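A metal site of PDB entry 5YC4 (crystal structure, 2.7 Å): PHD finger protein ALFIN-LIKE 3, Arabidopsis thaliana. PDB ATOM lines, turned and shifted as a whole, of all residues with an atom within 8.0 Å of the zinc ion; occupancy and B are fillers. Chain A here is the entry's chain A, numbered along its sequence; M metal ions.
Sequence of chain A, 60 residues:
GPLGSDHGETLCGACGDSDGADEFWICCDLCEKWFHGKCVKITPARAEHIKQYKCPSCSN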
ATOM      1  N   CYS A  27       2.917   7.065 -11.434  1.00  0.00           N
ATOM      2  CA  CYS A  27       2.312   6.396 -10.297  1.00  0.00           C
ATOM      3  C   CYS A  27       1.288   7.283  -9.593  1.00  0.00           C
ATOM      4  O   CYS A  27       1.519   8.473  -9.398  1.00  0.00           O
ATOM      5  CB  CYS A  27       3.392   5.961  -9.303  1.00  0.00           C
ATOM      6  SG  CYS A  27       2.833   4.841  -7.994  1.00  0.00           S
ATOM      7  N   CYS A  28       0.155   6.699  -9.233  1.00  0.00           N
ATOM      8  CA  CYS A  28      -0.852   7.411  -8.469  1.00  0.00           C
ATOM      9  C   CYS A  28      -0.392   7.593  -7.027  1.00  0.00           C
ATOM     10  O   CYS A  28       0.094   6.649  -6.406  1.00  0.00           O
ATOM     11  CB  CYS A  28      -2.194   6.669  -8.519  1.00  0.00           C
ATOM     12  SG  CYS A  28      -3.503   7.450  -7.539  1.00  0.00           S
ATOM     13  N   ASP A  29      -0.547   8.799  -6.493  1.00  0.00           N
ATOM     14  CA  ASP A  29      -0.051   9.097  -5.152  1.00  0.00           C
ATOM     15  C   ASP A  29      -1.000   8.635  -4.044  1.00  0.00           C
ATOM     16  O   ASP A  29      -0.664   8.707  -2.869  1.00  0.00           O
ATOM     17  CB  ASP A  29       0.202  10.601  -5.003  1.00  0.00           C
ATOM     18  CG  ASP A  29       1.552  11.019  -5.554  1.00  0.00           C
ATOM     19  OD1 ASP A  29       2.436  10.152  -5.695  1.00  0.00           O
ATOM     20  OD2 ASP A  29       1.733  12.222  -5.830  1.00  0.00           O
ATOM     21  N   LEU A  30      -2.178   8.149  -4.433  1.00  0.00           N
ATOM     22  CA  LEU A  30      -3.178   7.753  -3.443  1.00  0.00           C
ATOM     23  C   LEU A  30      -3.273   6.244  -3.257  1.00  0.00           C
ATOM     24  O   LEU A  30      -3.382   5.756  -2.134  1.00  0.00           O
ATOM     25  CB  LEU A  30      -4.548   8.321  -3.827  1.00  0.00           C
ATOM     26  CG  LEU A  30      -4.656   9.839  -3.749  1.00  0.00           C
ATOM     27  CD1 LEU A  30      -6.120  10.271  -3.776  1.00  0.00           C
ATOM     28  CD2 LEU A  30      -3.955  10.379  -2.514  1.00  0.00           C
ATOM     29  N   CYS A  31      -3.244   5.504  -4.358  1.00  0.00           N
ATOM     30  CA  CYS A  31      -3.348   4.047  -4.291  1.00  0.00           C
ATOM     31  C   CYS A  31      -2.028   3.377  -4.663  1.00  0.00           C
ATOM     32  O   CYS A  31      -1.895   2.152  -4.567  1.00  0.00           O
ATOM     33  CB  CYS A  31      -4.471   3.542  -5.204  1.00  0.00           C
ATOM     34  SG  CYS A  31      -4.087   3.581  -6.964  1.00  0.00           S
ATOM     35  N   GLU A  32      -1.069   4.187  -5.095  1.00  0.00           N
ATOM     36  CA  GLU A  32       0.288   3.741  -5.424  1.00  0.00           C
ATOM     37  C   GLU A  32       0.350   2.669  -6.510  1.00  0.00           C
ATOM     38  O   GLU A  32       1.237   1.822  -6.506  1.00  0.00           O
ATOM     39  CB  GLU A  32       0.988   3.231  -4.153  1.00  0.00           C
ATOM     40  CG  GLU A  32       1.286   4.326  -3.149  1.00  0.00           C
ATOM     41  CD  GLU A  32       2.067   3.828  -1.948  1.00  0.00           C
ATOM     42  OE1 GLU A  32       1.492   3.053  -1.148  1.00  0.00           O
ATOM     43  OE2 GLU A  32       3.243   4.215  -1.797  1.00  0.00           O
ATOM     44  N   LYS A  33      -0.602   2.724  -7.440  1.00  0.00           N
ATOM     45  CA  LYS A  33      -0.549   1.870  -8.626  1.00  0.00           C
ATOM     46  C   LYS A  33       0.236   2.555  -9.738  1.00  0.00           C
ATOM     47  O   LYS A  33       0.252   3.784  -9.833  1.00  0.00           O
ATOM     48  CB  LYS A  33      -1.960   1.529  -9.112  1.00  0.00           C
ATOM     49  CG  LYS A  33      -2.735   0.572  -8.223  1.00  0.00           C
ATOM     50  CD  LYS A  33      -4.116   0.307  -8.779  1.00  0.00           C
ATOM     51  CE  LYS A  33      -4.945  -0.569  -7.844  1.00  0.00           C
ATOM     52  NZ  LYS A  33      -6.358  -0.692  -8.300  1.00  0.00           N
ATOM     53  N   TRP A  34       0.894   1.752 -10.573  1.00  0.00           N
ATOM     54  CA  TRP A  34       1.644   2.289 -11.699  1.00  0.00           C
ATOM     55  C   TRP A  34       0.862   2.128 -12.995  1.00  0.00           C
ATOM     56  O   TRP A  34       0.078   1.196 -13.162  1.00  0.00           O
ATOM     57  CB  TRP A  34       2.996   1.586 -11.824  1.00  0.00           C
ATOM     58  CG  TRP A  34       4.044   2.109 -10.886  1.00  0.00           C
ATOM     59  CD1 TRP A  34       4.370   1.594  -9.663  1.00  0.00           C
ATOM     60  CD2 TRP A  34       4.902   3.236 -11.089  1.00  0.00           C
ATOM     61  NE1 TRP A  34       5.377   2.335  -9.091  1.00  0.00           N
ATOM     62  CE2 TRP A  34       5.718   3.350  -9.944  1.00  0.00           C
ATOM     63  CE3 TRP A  34       5.055   4.159 -12.127  1.00  0.00           C
ATOM     64  CZ2 TRP A  34       6.684   4.350  -9.814  1.00  0.00           C
ATOM     65  CZ3 TRP A  34       6.018   5.156 -11.988  1.00  0.00           C
ATOM     66  CH2 TRP A  34       6.815   5.239 -10.845  1.00  0.00           C
ATOM     67  N   PHE A  35       1.092   3.065 -13.921  1.00  0.00           N
ATOM     68  CA  PHE A  35       0.398   3.055 -15.198  1.00  0.00           C
ATOM     69  C   PHE A  35       1.341   3.429 -16.338  1.00  0.00           C
ATOM     70  O   PHE A  35       2.229   4.264 -16.154  1.00  0.00           O
ATOM     71  CB  PHE A  35      -0.787   4.036 -15.181  1.00  0.00           C
ATOM     72  CG  PHE A  35      -1.762   3.783 -14.063  1.00  0.00           C
ATOM     73  CD1 PHE A  35      -1.585   4.374 -12.820  1.00  0.00           C
ATOM     74  CD2 PHE A  35      -2.875   2.976 -14.265  1.00  0.00           C
ATOM     75  CE1 PHE A  35      -2.486   4.142 -11.793  1.00  0.00           C
ATOM     76  CE2 PHE A  35      -3.781   2.754 -13.237  1.00  0.00           C
ATOM     77  CZ  PHE A  35      -3.584   3.332 -12.001  1.00  0.00           C
ATOM     78  N   TYR A  53      -0.145  12.961  -9.051  1.00  0.00           N
ATOM     79  CA  TYR A  53      -1.040  12.228  -9.941  1.00  0.00           C
ATOM     80  C   TYR A  53      -2.053  11.391  -9.168  1.00  0.00           C
ATOM     81  O   TYR A  53      -1.708  10.671  -8.234  1.00  0.00           O
ATOM     82  CB  TYR A  53      -0.255  11.319 -10.892  1.00  0.00           C
ATOM     83  CG  TYR A  53      -1.154  10.508 -11.802  1.00  0.00           C
ATOM     84  CD1 TYR A  53      -1.970  11.148 -12.722  1.00  0.00           C
ATOM     85  CD2 TYR A  53      -1.201   9.122 -11.722  1.00  0.00           C
ATOM     86  CE1 TYR A  53      -2.811  10.424 -13.551  1.00  0.00           C
ATOM     87  CE2 TYR A  53      -2.029   8.392 -12.548  1.00  0.00           C
ATOM     88  CZ  TYR A  53      -2.831   9.049 -13.461  1.00  0.00           C
ATOM     89  OH  TYR A  53      -3.661   8.330 -14.296  1.00  0.00           O
ATOM     90  N   LYS A  54      -3.311  11.516  -9.583  1.00  0.00           N
ATOM     91  CA  LYS A  54      -4.401  10.771  -8.981  1.00  0.00           C
ATOM     92  C   LYS A  54      -5.135   9.978 -10.062  1.00  0.00           C
ATOM     93  O   LYS A  54      -5.815  10.565 -10.913  1.00  0.00           O
ATOM     94  CB  LYS A  54      -5.356  11.710  -8.244  1.00  0.00           C
ATOM     95  CG  LYS A  54      -6.573  11.048  -7.617  1.00  0.00           C
ATOM     96  CD  LYS A  54      -7.318  12.026  -6.723  1.00  0.00           C
ATOM     97  CE  LYS A  54      -7.585  13.350  -7.434  1.00  0.00           C
ATOM     98  NZ  LYS A  54      -8.200  14.355  -6.517  1.00  0.00           N
ATOM     99  N   CYS A  55      -4.980   8.660 -10.036  1.00  0.00           N
ATOM    100  CA  CYS A  55      -5.522   7.774 -11.061  1.00  0.00           C
ATOM    101  C   CYS A  55      -7.051   7.917 -11.167  1.00  0.00           C
ATOM    102  O   CYS A  55      -7.692   8.327 -10.208  1.00  0.00           O
ATOM    103  CB  CYS A  55      -5.144   6.322 -10.755  1.00  0.00           C
ATOM    104  SG  CYS A  55      -6.253   5.469  -9.607  1.00  0.00           S
ATOM    105  N   PRO A  56      -7.609   7.583 -12.342  1.00  0.00           N
ATOM    106  CA  PRO A  56      -9.058   7.678 -12.596  1.00  0.00           C
ATOM    107  C   PRO A  56      -9.928   7.013 -11.525  1.00  0.00           C
ATOM    108  O   PRO A  56     -11.009   7.514 -11.220  1.00  0.00           O
ATOM    109  CB  PRO A  56      -9.221   6.961 -13.940  1.00  0.00           C
ATOM    110  CG  PRO A  56      -7.925   7.178 -14.630  1.00  0.00           C
ATOM    111  CD  PRO A  56      -6.883   7.150 -13.549  1.00  0.00           C
ATOM    112  N   SER A  57      -9.450   5.905 -10.967  1.00  0.00           N
ATOM    113  CA  SER A  57     -10.205   5.198  -9.937  1.00  0.00           C
ATOM    114  C   SER A  57     -10.280   6.009  -8.651  1.00  0.00           C
ATOM    115  O   SER A  57     -11.321   6.025  -7.979  1.00  0.00           O
ATOM    116  CB  SER A  57      -9.566   3.829  -9.673  1.00  0.00           C
ATOM    117  OG  SER A  57     -10.377   3.066  -8.790  1.00  0.00           O
ATOM    118  N   CYS A  58      -9.192   6.689  -8.305  1.00  0.00           N
ATOM    119  CA  CYS A  58      -9.142   7.501  -7.100  1.00  0.00           C
ATOM    120  C   CYS A  58      -9.760   8.877  -7.335  1.00  0.00           C
ATOM    121  O   CYS A  58      -9.894   9.675  -6.411  1.00  0.00           O
ATOM    122  CB  CYS A  58      -7.698   7.658  -6.615  1.00  0.00           C
ATOM    123  SG  CYS A  58      -6.933   6.117  -6.045  1.00  0.00           S
ATOM    124  N   SER A  59     -10.144   9.144  -8.582  1.00  0.00           N
ATOM    125  CA  SER A  59     -10.727  10.437  -8.933  1.00  0.00           C
ATOM    126  C   SER A  59     -12.246  10.379  -8.988  1.00  0.00           C
ATOM    127  O   SER A  59     -12.889  11.137  -9.711  1.00  0.00           O
ATOM    128  CB  SER A  59     -10.179  10.901 -10.287  1.00  0.00           C
ATOM    129  OG  SER A  59      -8.768  11.044 -10.254  1.00  0.00           O
HETATM  130 ZN    ZN M   1      -5.124   5.605  -7.552  1.00  0.00          ZN
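SG of Cys 28 sits close to O of Tyr 53 (3.8 Å). The backbone NH of Leu 30 lies close to the side-chain sulfur of Cys 28. O of Lys 33 sits at hydrogen-bond distance from N of Cys 28, at 3.0 Å. SG of Cys 55 sits close to N of Ser 57 (3.5 Å). The backbone carbonyl oxygen (O) of Cys 55 sits at hydrogen-bond distance from the side-chain hydroxyl (OG) of Ser 59, at 2.9 Å. The side-chain sulfur (SG) of Cys 31 lies close to the backbone NH (N) of Lys 33.
Four residues have an atom within 4 Å of the zinc ion: Cys 28, Cys 31, Cys 55 and Cys 58.
SG of Cys 31 binds the zinc ion (2.3 Å). The zinc ion is bound by SG of Cys 55 (2.3 Å). SG of Cys 58 is bound to the zinc ion, at 2.4 Å. The side-chain sulfur (SG) of Cys 28 is bound to the zinc ion.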
